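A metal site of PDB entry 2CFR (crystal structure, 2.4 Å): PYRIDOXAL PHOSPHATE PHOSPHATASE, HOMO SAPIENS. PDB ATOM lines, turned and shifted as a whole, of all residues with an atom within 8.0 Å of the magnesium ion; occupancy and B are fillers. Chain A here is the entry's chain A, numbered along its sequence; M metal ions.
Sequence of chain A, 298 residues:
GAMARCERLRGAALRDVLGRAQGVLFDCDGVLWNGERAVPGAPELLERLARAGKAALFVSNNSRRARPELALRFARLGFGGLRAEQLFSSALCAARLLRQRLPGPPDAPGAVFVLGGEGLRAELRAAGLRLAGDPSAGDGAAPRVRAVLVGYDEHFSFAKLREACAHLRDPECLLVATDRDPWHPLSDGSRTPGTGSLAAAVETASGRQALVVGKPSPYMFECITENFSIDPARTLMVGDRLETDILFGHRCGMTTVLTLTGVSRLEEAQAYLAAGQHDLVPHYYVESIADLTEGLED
The side-chain carboxylate (OD2) of Asp 245 lies within hydrogen-bond range of the backbone NH (N) of Asp 240, at 3.2 Å.
The side-chain carboxylate of Asp 27 lies within salt-bridge range of the side-chain amino group of Lys 215, at 3.1 Å.
The side-chain carboxylate of Asp 240 sits at hydrogen-bond distance from the backbone NH of Val 263.
The side-chain carboxylate (OD1) of Asp 29 sits at hydrogen-bond distance from the indole nitrogen (NE1) of Trp 33.
N of Asp 27 lies within hydrogen-bond range of O of Val 238, at 2.9 Å.
The magnesium ion is bound by the side-chain carboxylate (OD2) of Asp 27 (2.1 Å), the side-chain carboxylate (OD1) of Asp 240 (2.2 Å) and the backbone carbonyl oxygen (O) of Asp 29 (2.4 Å).
The magnesium ion has three donor atoms within binding distance.
The nearest printed residue that does not touch the magnesium ion is Asp 245 (4.1 Å).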
ATOM      1  N   PHE A  26      14.211   8.643  23.217  1.00  0.00           N
ATOM      2  CA  PHE A  26      13.184   8.143  22.327  1.00  0.00           C
ATOM      3  C   PHE A  26      13.818   7.595  21.052  1.00  0.00           C
ATOM      4  O   PHE A  26      14.527   8.323  20.352  1.00  0.00           O
ATOM      5  CB  PHE A  26      12.220   9.261  21.896  1.00  0.00           C
ATOM      6  CG  PHE A  26      11.257   9.705  22.966  1.00  0.00           C
ATOM      7  CD1 PHE A  26      10.107   8.958  23.246  1.00  0.00           C
ATOM      8  CD2 PHE A  26      11.493  10.897  23.664  1.00  0.00           C
ATOM      9  CE1 PHE A  26       9.204   9.387  24.237  1.00  0.00           C
ATOM     10  CE2 PHE A  26      10.610  11.315  24.647  1.00  0.00           C
ATOM     11  CZ  PHE A  26       9.470  10.580  24.934  1.00  0.00           C
ATOM     12  N   ASP A  27      13.555   6.322  20.769  1.00  0.00           N
ATOM     13  CA  ASP A  27      13.610   5.835  19.417  1.00  0.00           C
ATOM     14  C   ASP A  27      12.639   6.700  18.566  1.00  0.00           C
ATOM     15  O   ASP A  27      11.779   7.372  19.131  1.00  0.00           O
ATOM     16  CB  ASP A  27      13.180   4.387  19.411  1.00  0.00           C
ATOM     17  CG  ASP A  27      13.027   3.859  18.032  1.00  0.00           C
ATOM     18  OD1 ASP A  27      13.933   4.070  17.212  1.00  0.00           O
ATOM     19  OD2 ASP A  27      11.993   3.257  17.748  1.00  0.00           O
ATOM     20  N   CYS A  28      12.749   6.702  17.244  1.00  0.00           N
ATOM     21  CA  CYS A  28      11.821   7.544  16.458  1.00  0.00           C
ATOM     22  C   CYS A  28      10.701   6.786  15.726  1.00  0.00           C
ATOM     23  O   CYS A  28       9.526   6.929  16.056  1.00  0.00           O
ATOM     24  CB  CYS A  28      12.576   8.467  15.493  1.00  0.00           C
ATOM     25  SG  CYS A  28      13.829   9.494  16.318  1.00  0.00           S
ATOM     26  N   ASP A  29      11.068   5.969  14.753  1.00  0.00           N
ATOM     27  CA  ASP A  29      10.098   5.213  13.955  1.00  0.00           C
ATOM     28  C   ASP A  29       9.462   4.101  14.761  1.00  0.00           C
ATOM     29  O   ASP A  29      10.135   3.372  15.498  1.00  0.00           O
ATOM     30  CB  ASP A  29      10.798   4.650  12.725  1.00  0.00           C
ATOM     31  CG  ASP A  29      11.678   5.674  12.041  1.00  0.00           C
ATOM     32  OD1 ASP A  29      11.159   6.707  11.556  1.00  0.00           O
ATOM     33  OD2 ASP A  29      12.916   5.450  12.005  1.00  0.00           O
ATOM     34  N   GLY A  30       8.142   3.978  14.622  1.00  0.00           N
ATOM     35  CA  GLY A  30       7.352   3.112  15.492  1.00  0.00           C
ATOM     36  C   GLY A  30       7.039   3.721  16.858  1.00  0.00           C
ATOM     37  O   GLY A  30       6.264   3.147  17.627  1.00  0.00           O
ATOM     38  N   VAL A  31       7.622   4.880  17.152  1.00  0.00           N
ATOM     39  CA  VAL A  31       7.510   5.502  18.488  1.00  0.00           C
ATOM     40  C   VAL A  31       6.816   6.842  18.418  1.00  0.00           C
ATOM     41  O   VAL A  31       5.758   7.030  19.014  1.00  0.00           O
ATOM     42  CB  VAL A  31       8.893   5.658  19.161  1.00  0.00           C
ATOM     43  CG1 VAL A  31       8.774   6.341  20.575  1.00  0.00           C
ATOM     44  CG2 VAL A  31       9.552   4.297  19.262  1.00  0.00           C
ATOM     45  N   LEU A  32       7.418   7.760  17.664  1.00  0.00           N
ATOM     46  CA  LEU A  32       6.867   9.094  17.434  1.00  0.00           C
ATOM     47  C   LEU A  32       5.928   9.113  16.245  1.00  0.00           C
ATOM     48  O   LEU A  32       4.991   9.928  16.184  1.00  0.00           O
ATOM     49  CB  LEU A  32       8.004  10.090  17.145  1.00  0.00           C
ATOM     50  CG  LEU A  32       9.128  10.201  18.144  1.00  0.00           C
ATOM     51  CD1 LEU A  32      10.097  11.230  17.631  1.00  0.00           C
ATOM     52  CD2 LEU A  32       8.636  10.503  19.570  1.00  0.00           C
ATOM     53  N   TRP A  33       6.198   8.217  15.296  1.00  0.00           N
ATOM     54  CA  TRP A  33       5.504   8.187  14.022  1.00  0.00           C
ATOM     55  C   TRP A  33       5.609   6.818  13.331  1.00  0.00           C
ATOM     56  O   TRP A  33       6.457   5.977  13.678  1.00  0.00           O
ATOM     57  CB  TRP A  33       6.033   9.305  13.096  1.00  0.00           C
ATOM     58  CG  TRP A  33       7.565   9.317  12.909  1.00  0.00           C
ATOM     59  CD1 TRP A  33       8.322   8.349  12.315  1.00  0.00           C
ATOM     60  CD2 TRP A  33       8.488  10.373  13.270  1.00  0.00           C
ATOM     61  NE1 TRP A  33       9.633   8.718  12.312  1.00  0.00           N
ATOM     62  CE2 TRP A  33       9.775   9.950  12.883  1.00  0.00           C
ATOM     63  CE3 TRP A  33       8.338  11.628  13.896  1.00  0.00           C
ATOM     64  CZ2 TRP A  33      10.938  10.740  13.087  1.00  0.00           C
ATOM     65  CZ3 TRP A  33       9.496  12.404  14.118  1.00  0.00           C
ATOM     66  CH2 TRP A  33      10.782  11.952  13.698  1.00  0.00           C
ATOM     67  N   ASN A  34       4.716   6.606  12.365  1.00  0.00           N
ATOM     68  CA  ASN A  34       4.750   5.444  11.471  1.00  0.00           C
ATOM     69  C   ASN A  34       4.529   5.973  10.062  1.00  0.00           C
ATOM     70  O   ASN A  34       3.424   6.465   9.730  1.00  0.00           O
ATOM     71  CB  ASN A  34       3.634   4.459  11.797  1.00  0.00           C
ATOM     72  CG  ASN A  34       3.929   3.598  13.006  1.00  0.00           C
ATOM     73  OD1 ASN A  34       4.909   2.852  13.023  1.00  0.00           O
ATOM     74  ND2 ASN A  34       3.074   3.683  14.022  1.00  0.00           N
ATOM     75  N   VAL A  59      17.289   8.739  19.547  1.00  0.00           N
ATOM     76  CA  VAL A  59      18.270   7.753  19.109  1.00  0.00           C
ATOM     77  C   VAL A  59      17.686   6.926  17.992  1.00  0.00           C
ATOM     78  O   VAL A  59      16.708   6.190  18.185  1.00  0.00           O
ATOM     79  CB  VAL A  59      18.760   6.826  20.250  1.00  0.00           C
ATOM     80  CG1 VAL A  59      20.013   6.114  19.867  1.00  0.00           C
ATOM     81  CG2 VAL A  59      19.052   7.624  21.444  1.00  0.00           C
ATOM     82  N   SER A  60      18.323   7.039  16.834  1.00  0.00           N
ATOM     83  CA  SER A  60      17.892   6.430  15.605  1.00  0.00           C
ATOM     84  C   SER A  60      19.051   5.625  14.968  1.00  0.00           C
ATOM     85  O   SER A  60      20.172   6.127  14.825  1.00  0.00           O
ATOM     86  CB  SER A  60      17.448   7.538  14.643  1.00  0.00           C
ATOM     87  OG  SER A  60      16.864   7.037  13.462  1.00  0.00           O
ATOM     88  N   ASN A  61      18.751   4.395  14.573  1.00  0.00           N
ATOM     89  CA  ASN A  61      19.662   3.555  13.790  1.00  0.00           C
ATOM     90  C   ASN A  61      19.687   3.927  12.314  1.00  0.00           C
ATOM     91  O   ASN A  61      20.328   3.241  11.508  1.00  0.00           O
ATOM     92  CB  ASN A  61      19.316   2.056  13.963  1.00  0.00           C
ATOM     93  CG  ASN A  61      19.902   1.457  15.218  1.00  0.00           C
ATOM     94  OD1 ASN A  61      20.723   2.071  15.907  1.00  0.00           O
ATOM     95  ND2 ASN A  61      19.504   0.226  15.527  1.00  0.00           N
ATOM     96  N   ASP A 181      19.819  -3.992  12.219  1.00  0.00           N
ATOM     97  CA  ASP A 181      18.393  -4.050  11.985  1.00  0.00           C
ATOM     98  C   ASP A 181      18.193  -4.899  10.732  1.00  0.00           C
ATOM     99  O   ASP A 181      18.635  -4.518   9.655  1.00  0.00           O
ATOM    100  CB  ASP A 181      17.820  -2.646  11.748  1.00  0.00           C
ATOM    101  CG  ASP A 181      17.688  -1.796  13.023  1.00  0.00           C
ATOM    102  OD1 ASP A 181      17.389  -0.602  12.866  1.00  0.00           O
ATOM    103  OD2 ASP A 181      17.829  -2.298  14.174  1.00  0.00           O
ATOM    104  N   HIS A 184      12.831  -3.469   7.904  1.00  0.00           N
ATOM    105  CA  HIS A 184      12.049  -2.302   8.321  1.00  0.00           C
ATOM    106  C   HIS A 184      10.677  -2.315   7.666  1.00  0.00           C
ATOM    107  O   HIS A 184      10.572  -2.575   6.466  1.00  0.00           O
ATOM    108  CB  HIS A 184      12.803  -1.013   7.950  1.00  0.00           C
ATOM    109  CG  HIS A 184      14.133  -0.882   8.627  1.00  0.00           C
ATOM    110  ND1 HIS A 184      14.252  -0.607   9.974  1.00  0.00           N
ATOM    111  CD2 HIS A 184      15.395  -1.054   8.159  1.00  0.00           C
ATOM    112  CE1 HIS A 184      15.531  -0.594  10.305  1.00  0.00           C
ATOM    113  NE2 HIS A 184      16.243  -0.860   9.225  1.00  0.00           N
ATOM    114  N   PRO A 185       9.615  -2.022   8.431  1.00  0.00           N
ATOM    115  CA  PRO A 185       8.258  -1.956   7.880  1.00  0.00           C
ATOM    116  C   PRO A 185       7.991  -0.703   7.041  1.00  0.00           C
ATOM    117  O   PRO A 185       8.573   0.360   7.287  1.00  0.00           O
ATOM    118  CB  PRO A 185       7.362  -1.930   9.127  1.00  0.00           C
ATOM    119  CG  PRO A 185       8.268  -2.217  10.307  1.00  0.00           C
ATOM    120  CD  PRO A 185       9.630  -1.766   9.881  1.00  0.00           C
ATOM    121  N   LYS A 215      22.166   0.971  18.277  1.00  0.00           N
ATOM    122  CA  LYS A 215      21.482   0.133  19.231  1.00  0.00           C
ATOM    123  C   LYS A 215      21.324  -1.241  18.618  1.00  0.00           C
ATOM    124  O   LYS A 215      21.096  -1.351  17.416  1.00  0.00           O
ATOM    125  CB  LYS A 215      20.098   0.706  19.532  1.00  0.00           C
ATOM    126  CG  LYS A 215      20.048   2.188  19.916  1.00  0.00           C
ATOM    127  CD  LYS A 215      18.606   2.672  19.839  1.00  0.00           C
ATOM    128  CE  LYS A 215      18.131   2.706  18.384  1.00  0.00           C
ATOM    129  NZ  LYS A 215      16.678   3.069  18.235  1.00  0.00           N
ATOM    130  N   MET A 237      14.218   4.888  28.516  1.00  0.00           N
ATOM    131  CA  MET A 237      14.471   4.545  27.121  1.00  0.00           C
ATOM    132  C   MET A 237      13.173   3.981  26.523  1.00  0.00           C
ATOM    133  O   MET A 237      12.614   3.006  27.035  1.00  0.00           O
ATOM    134  CB  MET A 237      15.662   3.576  26.994  1.00  0.00           C
ATOM    135  CG  MET A 237      15.848   2.951  25.610  1.00  0.00           C
ATOM    136  SD  MET A 237      16.477   4.242  24.286  1.00  0.00           S
ATOM    137  CE  MET A 237      15.620   3.576  22.670  1.00  0.00           C
ATOM    138  N   VAL A 238      12.684   4.620  25.467  1.00  0.00           N
ATOM    139  CA  VAL A 238      11.384   4.296  24.921  1.00  0.00           C
ATOM    140  C   VAL A 238      11.603   3.865  23.485  1.00  0.00           C
ATOM    141  O   VAL A 238      12.211   4.585  22.713  1.00  0.00           O
ATOM    142  CB  VAL A 238      10.378   5.527  24.986  1.00  0.00           C
ATOM    143  CG1 VAL A 238       9.008   5.154  24.472  1.00  0.00           C
ATOM    144  CG2 VAL A 238      10.298   6.158  26.408  1.00  0.00           C
ATOM    145  N   GLY A 239      11.111   2.678  23.135  1.00  0.00           N
ATOM    146  CA  GLY A 239      11.209   2.181  21.767  1.00  0.00           C
ATOM    147  C   GLY A 239      10.170   1.130  21.424  1.00  0.00           C
ATOM    148  O   GLY A 239       9.459   0.667  22.297  1.00  0.00           O
ATOM    149  N   ASP A 240      10.094   0.739  20.154  1.00  0.00           N
ATOM    150  CA  ASP A 240       9.156  -0.264  19.718  1.00  0.00           C
ATOM    151  C   ASP A 240       9.752  -1.683  19.469  1.00  0.00           C
ATOM    152  O   ASP A 240       8.988  -2.654  19.296  1.00  0.00           O
ATOM    153  CB  ASP A 240       8.453   0.215  18.458  1.00  0.00           C
ATOM    154  CG  ASP A 240       9.389   0.319  17.269  1.00  0.00           C
ATOM    155  OD1 ASP A 240      10.356   1.112  17.299  1.00  0.00           O
ATOM    156  OD2 ASP A 240       9.140  -0.363  16.257  1.00  0.00           O
ATOM    157  N   ARG A 241      11.088  -1.799  19.441  1.00  0.00           N
ATOM    158  CA  ARG A 241      11.762  -3.041  19.077  1.00  0.00           C
ATOM    159  C   ARG A 241      12.516  -3.599  20.255  1.00  0.00           C
ATOM    160  O   ARG A 241      13.505  -3.013  20.696  1.00  0.00           O
ATOM    161  CB  ARG A 241      12.775  -2.831  17.946  1.00  0.00           C
ATOM    162  CG  ARG A 241      12.252  -2.835  16.562  1.00  0.00           C
ATOM    163  CD  ARG A 241      13.048  -3.818  15.694  1.00  0.00           C
ATOM    164  NE  ARG A 241      13.153  -3.338  14.318  1.00  0.00           N
ATOM    165  CZ  ARG A 241      13.219  -4.105  13.228  1.00  0.00           C
ATOM    166  NH1 ARG A 241      13.168  -5.433  13.294  1.00  0.00           N
ATOM    167  NH2 ARG A 241      13.322  -3.513  12.050  1.00  0.00           N
ATOM    168  N   THR A 244      16.366  -4.221  19.773  1.00  0.00           N
ATOM    169  CA  THR A 244      17.106  -2.993  19.490  1.00  0.00           C
ATOM    170  C   THR A 244      17.080  -1.994  20.674  1.00  0.00           C
ATOM    171  O   THR A 244      18.098  -1.736  21.305  1.00  0.00           O
ATOM    172  CB  THR A 244      16.533  -2.346  18.246  1.00  0.00           C
ATOM    173  OG1 THR A 244      16.663  -3.258  17.149  1.00  0.00           O
ATOM    174  CG2 THR A 244      17.243  -1.053  17.921  1.00  0.00           C
ATOM    175  N   ASP A 245      15.899  -1.451  20.977  1.00  0.00           N
ATOM    176  CA  ASP A 245      15.740  -0.369  21.938  1.00  0.00           C
ATOM    177  C   ASP A 245      15.660  -0.883  23.325  1.00  0.00           C
ATOM    178  O   ASP A 245      16.286  -0.330  24.229  1.00  0.00           O
ATOM    179  CB  ASP A 245      14.449   0.404  21.652  1.00  0.00           C
ATOM    180  CG  ASP A 245      14.281   0.704  20.228  1.00  0.00           C
ATOM    181  OD1 ASP A 245      15.270   1.191  19.640  1.00  0.00           O
ATOM    182  OD2 ASP A 245      13.210   0.416  19.672  1.00  0.00           O
ATOM    183  N   THR A 259       6.651   0.697  23.558  1.00  0.00           N
ATOM    184  CA  THR A 259       5.485   1.313  22.982  1.00  0.00           C
ATOM    185  C   THR A 259       4.983   0.367  21.871  1.00  0.00           C
ATOM    186  O   THR A 259       5.795  -0.267  21.175  1.00  0.00           O
ATOM    187  CB  THR A 259       5.768   2.756  22.517  1.00  0.00           C
ATOM    188  OG1 THR A 259       4.548   3.388  22.144  1.00  0.00           O
ATOM    189  CG2 THR A 259       6.669   2.773  21.345  1.00  0.00           C
ATOM    190  N   GLY A 262       4.808   0.119  17.057  1.00  0.00           N
ATOM    191  CA  GLY A 262       5.819  -0.282  16.091  1.00  0.00           C
ATOM    192  C   GLY A 262       5.975  -1.777  15.898  1.00  0.00           C
ATOM    193  O   GLY A 262       5.003  -2.484  15.746  1.00  0.00           O
ATOM    194  N   VAL A 263       7.219  -2.241  15.893  1.00  0.00           N
ATOM    195  CA  VAL A 263       7.572  -3.588  15.429  1.00  0.00           C
ATOM    196  C   VAL A 263       7.220  -4.744  16.412  1.00  0.00           C
ATOM    197  O   VAL A 263       6.599  -5.744  16.017  1.00  0.00           O
ATOM    198  CB  VAL A 263       9.063  -3.644  14.983  1.00  0.00           C
ATOM    199  CG1 VAL A 263       9.486  -5.085  14.616  1.00  0.00           C
ATOM    200  CG2 VAL A 263       9.311  -2.686  13.790  1.00  0.00           C
HETATM  201 MG    MG M   1      12.013   2.026  16.091  1.00  0.00          MG
